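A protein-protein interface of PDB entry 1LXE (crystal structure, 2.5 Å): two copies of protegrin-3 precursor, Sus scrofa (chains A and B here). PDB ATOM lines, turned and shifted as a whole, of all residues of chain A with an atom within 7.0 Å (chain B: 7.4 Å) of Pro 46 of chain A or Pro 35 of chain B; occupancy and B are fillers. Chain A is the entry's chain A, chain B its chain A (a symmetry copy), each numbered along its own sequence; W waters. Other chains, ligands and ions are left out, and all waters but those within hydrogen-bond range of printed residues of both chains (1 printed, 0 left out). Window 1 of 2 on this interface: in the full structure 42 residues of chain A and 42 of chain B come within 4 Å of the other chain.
The backbone NH of Val 47 of chain A sits at hydrogen-bond distance from the backbone carbonyl oxygen of Gly 80 of chain A (3.0 Å).
Of the printed residues of chain A, Pro 35 of chain B touches Pro 46 (3.98 Å) and Ser 48 (3.9 Å). Of the printed residues of chain A, Asp 32 of chain B touches Ser 48 (2.6 Å). Printed residues of chain A within 4 Å of Tyr 5 of chain B: Pro 46 and Val 47. Of the printed residues of chain B, Val 47 of chain A touches Tyr 5 (3.3 Å). Printed residues of chain B within 4 Å of Ser 48 of chain A: Asp 32 (2.6 Å) and Pro 35 (3.9 Å). Asp 38 of chain B touches none of the printed residues of chain A. The nearest printed residue of chain B that does not touch Pro 46 of chain A is Pro 34 of chain B (4.5 Å). The nearest printed residue of chain A that does not touch Pro 35 of chain B is Val 47 of chain A (4.2 Å). The nearest printed residue of chain A that does not touch Tyr 5 of chain B is Ser 48 of chain A (4.4 Å).
CG of Pro 35 of chain B touches CB of Pro 46 of chain A (3.98 Å). Val 47 of chain A touches Tyr 5 of chain B. Ser 48 of chain A touches Pro 35 of chain B.
Water W1 lies within hydrogen-bond range of the backbone carbonyl oxygen (O) of Asp 32 of chain B (2.7 Å), the backbone NH (N) of Ser 48 of chain A (2.7 Å) and the side-chain hydroxyl (OH) of Tyr 5 of chain B (2.8 Å).
Hydrophobic or aromatic side chains of chain B that line the printed part of chain A: Tyr 5 and Pro 35. Of the 10 printed residues of chain A, 3 touch a printed residue of chain B. Hydrophobic or aromatic side chains of chain A within 4 Å of the printed part of chain B: Pro 46 and Val 47. Among the printed residues, 5 pairs touch across the chains. Among the printed residues, no Asp or Glu carboxylate lies within 4 Å of a Lys or Arg side-chain nitrogen of the other chain.
No position is printed for both chains. Of the 5 pairs that touch across the chains among the printed residues, none has its exchanged pair printed and touching as well.
The backbone NH (N) of Asp 32 of chain B is in hydrogen-bond range of the backbone carbonyl oxygen (O) of Ser 48 of chain A, 2.6 Å away. OH of Tyr 5 of chain B lies within hydrogen-bond range of O of Pro 46 of chain A, 3.2 Å away.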
ATOM      1  N   THR A  43      33.518   2.663  19.521  1.00  0.00           N
ATOM      2  CA  THR A  43      33.329   1.792  18.373  1.00  0.00           C
ATOM      3  C   THR A  43      32.086   2.221  17.608  1.00  0.00           C
ATOM      4  O   THR A  43      31.224   2.922  18.145  1.00  0.00           O
ATOM      5  CB  THR A  43      33.165   0.323  18.802  1.00  0.00           C
ATOM      6  OG1 THR A  43      32.229   0.237  19.880  1.00  0.00           O
ATOM      7  CG2 THR A  43      34.489  -0.252  19.244  1.00  0.00           C
ATOM      8  N   PRO A  44      31.976   1.801  16.341  1.00  0.00           N
ATOM      9  CA  PRO A  44      30.818   2.168  15.533  1.00  0.00           C
ATOM     10  C   PRO A  44      29.529   1.673  16.161  1.00  0.00           C
ATOM     11  O   PRO A  44      29.457   0.551  16.648  1.00  0.00           O
ATOM     12  CB  PRO A  44      31.114   1.507  14.196  1.00  0.00           C
ATOM     13  CG  PRO A  44      32.621   1.549  14.133  1.00  0.00           C
ATOM     14  CD  PRO A  44      32.970   1.084  15.526  1.00  0.00           C
ATOM     15  N   LYS A  45      28.513   2.527  16.173  1.00  0.00           N
ATOM     16  CA  LYS A  45      27.251   2.147  16.748  1.00  0.00           C
ATOM     17  C   LYS A  45      26.303   1.833  15.602  1.00  0.00           C
ATOM     18  O   LYS A  45      26.375   2.451  14.533  1.00  0.00           O
ATOM     19  CB  LYS A  45      26.704   3.280  17.618  1.00  0.00           C
ATOM     20  CG  LYS A  45      27.665   3.773  18.720  1.00  0.00           C
ATOM     21  CD  LYS A  45      28.039   2.688  19.735  1.00  0.00           C
ATOM     22  CE  LYS A  45      29.126   3.158  20.703  1.00  0.00           C
ATOM     23  NZ  LYS A  45      29.806   2.015  21.393  1.00  0.00           N
ATOM     24  N   PRO A  46      25.434   0.833  15.791  1.00  0.00           N
ATOM     25  CA  PRO A  46      24.466   0.438  14.766  1.00  0.00           C
ATOM     26  C   PRO A  46      23.310   1.441  14.639  1.00  0.00           C
ATOM     27  O   PRO A  46      22.969   2.133  15.591  1.00  0.00           O
ATOM     28  CB  PRO A  46      24.004  -0.938  15.242  1.00  0.00           C
ATOM     29  CG  PRO A  46      24.121  -0.834  16.744  1.00  0.00           C
ATOM     30  CD  PRO A  46      25.440  -0.120  16.918  1.00  0.00           C
ATOM     31  N   VAL A  47      22.732   1.523  13.444  1.00  0.00           N
ATOM     32  CA  VAL A  47      21.618   2.422  13.177  1.00  0.00           C
ATOM     33  C   VAL A  47      20.610   1.786  12.231  1.00  0.00           C
ATOM     34  O   VAL A  47      20.936   0.902  11.447  1.00  0.00           O
ATOM     35  CB  VAL A  47      22.103   3.744  12.548  1.00  0.00           C
ATOM     36  CG1 VAL A  47      23.051   4.441  13.492  1.00  0.00           C
ATOM     37  CG2 VAL A  47      22.800   3.470  11.229  1.00  0.00           C
ATOM     38  N   SER A  48      19.373   2.240  12.319  1.00  0.00           N
ATOM     39  CA  SER A  48      18.319   1.739  11.460  1.00  0.00           C
ATOM     40  C   SER A  48      17.333   2.887  11.300  1.00  0.00           C
ATOM     41  O   SER A  48      16.823   3.428  12.280  1.00  0.00           O
ATOM     42  CB  SER A  48      17.631   0.525  12.101  1.00  0.00           C
ATOM     43  OG  SER A  48      16.590   0.016  11.281  1.00  0.00           O
ATOM     44  N   VAL A  79      20.256   0.185   7.008  1.00  0.00           N
ATOM     45  CA  VAL A  79      20.851  -0.397   8.200  1.00  0.00           C
ATOM     46  C   VAL A  79      22.346  -0.364   8.006  1.00  0.00           C
ATOM     47  O   VAL A  79      22.840  -0.525   6.889  1.00  0.00           O
ATOM     48  CB  VAL A  79      20.415  -1.849   8.423  1.00  0.00           C
ATOM     49  CG1 VAL A  79      18.917  -1.903   8.731  1.00  0.00           C
ATOM     50  CG2 VAL A  79      20.730  -2.668   7.191  1.00  0.00           C
ATOM     51  N   GLY A  80      23.062  -0.138   9.102  1.00  0.00           N
ATOM     52  CA  GLY A  80      24.508  -0.083   9.051  1.00  0.00           C
ATOM     53  C   GLY A  80      25.067   0.439  10.352  1.00  0.00           C
ATOM     54  O   GLY A  80      24.480   0.237  11.419  1.00  0.00           O
ATOM     55  N   THR A  81      26.201   1.125  10.269  1.00  0.00           N
ATOM     56  CA  THR A  81      26.820   1.680  11.458  1.00  0.00           C
ATOM     57  C   THR A  81      27.418   3.073  11.205  1.00  0.00           C
ATOM     58  O   THR A  81      27.737   3.436  10.066  1.00  0.00           O
ATOM     59  CB  THR A  81      27.948   0.753  11.984  1.00  0.00           C
ATOM     60  OG1 THR A  81      29.071   0.818  11.102  1.00  0.00           O
ATOM     61  CG2 THR A  81      27.476  -0.693  12.063  1.00  0.00           C
ATOM     62  N   VAL A  82      27.559   3.840  12.284  1.00  0.00           N
ATOM     63  CA  VAL A  82      28.149   5.172  12.236  1.00  0.00           C
ATOM     64  C   VAL A  82      29.160   5.311  13.384  1.00  0.00           C
ATOM     65  O   VAL A  82      28.931   4.817  14.489  1.00  0.00           O
ATOM     66  CB  VAL A  82      27.073   6.269  12.391  1.00  0.00           C
ATOM     67  CG1 VAL A  82      26.169   6.288  11.174  1.00  0.00           C
ATOM     68  CG2 VAL A  82      26.248   6.016  13.653  1.00  0.00           C
ATOM     69  N   TYR B   5      24.359  11.122  18.029  1.00  0.00           N
ATOM     70  CA  TYR B   5      23.876   9.907  17.385  1.00  0.00           C
ATOM     71  C   TYR B   5      22.981  10.343  16.214  1.00  0.00           C
ATOM     72  O   TYR B   5      23.251  10.017  15.040  1.00  0.00           O
ATOM     73  CB  TYR B   5      23.049   9.074  18.371  1.00  0.00           C
ATOM     74  CG  TYR B   5      22.435   7.848  17.740  1.00  0.00           C
ATOM     75  CD1 TYR B   5      23.246   6.819  17.258  1.00  0.00           C
ATOM     76  CD2 TYR B   5      21.046   7.728  17.583  1.00  0.00           C
ATOM     77  CE1 TYR B   5      22.700   5.699  16.632  1.00  0.00           C
ATOM     78  CE2 TYR B   5      20.487   6.607  16.957  1.00  0.00           C
ATOM     79  CZ  TYR B   5      21.327   5.597  16.485  1.00  0.00           C
ATOM     80  OH  TYR B   5      20.817   4.480  15.864  1.00  0.00           O
ATOM     81  N   VAL B   9      23.219  10.297  11.988  1.00  0.00           N
ATOM     82  CA  VAL B   9      22.269   9.729  11.037  1.00  0.00           C
ATOM     83  C   VAL B   9      22.016  10.717   9.900  1.00  0.00           C
ATOM     84  O   VAL B   9      21.897  10.327   8.740  1.00  0.00           O
ATOM     85  CB  VAL B   9      20.945   9.372  11.731  1.00  0.00           C
ATOM     86  CG1 VAL B   9      19.896   8.954  10.710  1.00  0.00           C
ATOM     87  CG2 VAL B   9      21.197   8.260  12.733  1.00  0.00           C
ATOM     88  N   ASP B  32      14.774   4.503  13.519  1.00  0.00           N
ATOM     89  CA  ASP B  32      14.328   3.345  14.288  1.00  0.00           C
ATOM     90  C   ASP B  32      15.180   3.076  15.505  1.00  0.00           C
ATOM     91  O   ASP B  32      16.130   3.802  15.784  1.00  0.00           O
ATOM     92  CB  ASP B  32      14.309   2.109  13.383  1.00  0.00           C
ATOM     93  CG  ASP B  32      13.533   2.351  12.096  1.00  0.00           C
ATOM     94  OD1 ASP B  32      12.296   2.464  12.175  1.00  0.00           O
ATOM     95  OD2 ASP B  32      14.153   2.450  11.009  1.00  0.00           O
ATOM     96  N   GLN B  33      14.825   2.028  16.239  1.00  0.00           N
ATOM     97  CA  GLN B  33      15.565   1.659  17.437  1.00  0.00           C
ATOM     98  C   GLN B  33      16.827   0.905  17.082  1.00  0.00           C
ATOM     99  O   GLN B  33      16.834   0.085  16.168  1.00  0.00           O
ATOM    100  CB  GLN B  33      14.729   0.776  18.363  1.00  0.00           C
ATOM    101  CG  GLN B  33      13.571   1.464  19.033  1.00  0.00           C
ATOM    102  CD  GLN B  33      12.979   0.610  20.131  1.00  0.00           C
ATOM    103  OE1 GLN B  33      12.756  -0.588  19.942  1.00  0.00           O
ATOM    104  NE2 GLN B  33      12.716   1.221  21.284  1.00  0.00           N
ATOM    105  N   PRO B  34      17.917   1.175  17.817  1.00  0.00           N
ATOM    106  CA  PRO B  34      19.199   0.510  17.580  1.00  0.00           C
ATOM    107  C   PRO B  34      18.991  -1.000  17.571  1.00  0.00           C
ATOM    108  O   PRO B  34      18.776  -1.606  18.621  1.00  0.00           O
ATOM    109  CB  PRO B  34      20.044   0.972  18.759  1.00  0.00           C
ATOM    110  CG  PRO B  34      19.512   2.354  19.020  1.00  0.00           C
ATOM    111  CD  PRO B  34      18.025   2.154  18.915  1.00  0.00           C
ATOM    112  N   PRO B  35      19.050  -1.626  16.380  1.00  0.00           N
ATOM    113  CA  PRO B  35      18.867  -3.075  16.234  1.00  0.00           C
ATOM    114  C   PRO B  35      19.665  -3.852  17.274  1.00  0.00           C
ATOM    115  O   PRO B  35      20.895  -3.788  17.307  1.00  0.00           O
ATOM    116  CB  PRO B  35      19.332  -3.342  14.802  1.00  0.00           C
ATOM    117  CG  PRO B  35      20.300  -2.223  14.536  1.00  0.00           C
ATOM    118  CD  PRO B  35      19.577  -1.046  15.135  1.00  0.00           C
ATOM    119  N   LYS B  36      18.945  -4.592  18.112  1.00  0.00           N
ATOM    120  CA  LYS B  36      19.535  -5.363  19.196  1.00  0.00           C
ATOM    121  C   LYS B  36      20.769  -6.200  18.886  1.00  0.00           C
ATOM    122  O   LYS B  36      20.796  -7.006  17.953  1.00  0.00           O
ATOM    123  CB  LYS B  36      18.459  -6.234  19.860  1.00  0.00           C
ATOM    124  CG  LYS B  36      17.575  -5.463  20.853  1.00  0.00           C
ATOM    125  CD  LYS B  36      16.960  -4.213  20.221  1.00  0.00           C
ATOM    126  CE  LYS B  36      16.287  -3.322  21.254  1.00  0.00           C
ATOM    127  NZ  LYS B  36      15.762  -2.060  20.644  1.00  0.00           N
ATOM    128  N   ALA B  37      21.794  -5.971  19.703  1.00  0.00           N
ATOM    129  CA  ALA B  37      23.070  -6.666  19.615  1.00  0.00           C
ATOM    130  C   ALA B  37      23.291  -7.277  20.994  1.00  0.00           C
ATOM    131  O   ALA B  37      23.293  -6.568  22.005  1.00  0.00           O
ATOM    132  CB  ALA B  37      24.176  -5.677  19.288  1.00  0.00           C
ATOM    133  N   ASP B  38      23.470  -8.591  21.036  1.00  0.00           N
ATOM    134  CA  ASP B  38      23.655  -9.289  22.301  1.00  0.00           C
ATOM    135  C   ASP B  38      24.892  -8.876  23.077  1.00  0.00           C
ATOM    136  O   ASP B  38      25.987  -8.753  22.521  1.00  0.00           O
ATOM    137  CB  ASP B  38      23.670 -10.809  22.077  1.00  0.00           C
ATOM    138  CG  ASP B  38      24.955 -11.463  22.547  1.00  0.00           C
ATOM    139  OD1 ASP B  38      26.005 -11.259  21.898  1.00  0.00           O
ATOM    140  OD2 ASP B  38      24.912 -12.180  23.569  1.00  0.00           O
HETATM  141  O   HOH W   1      18.514   3.487  14.602  1.00  0.00           O
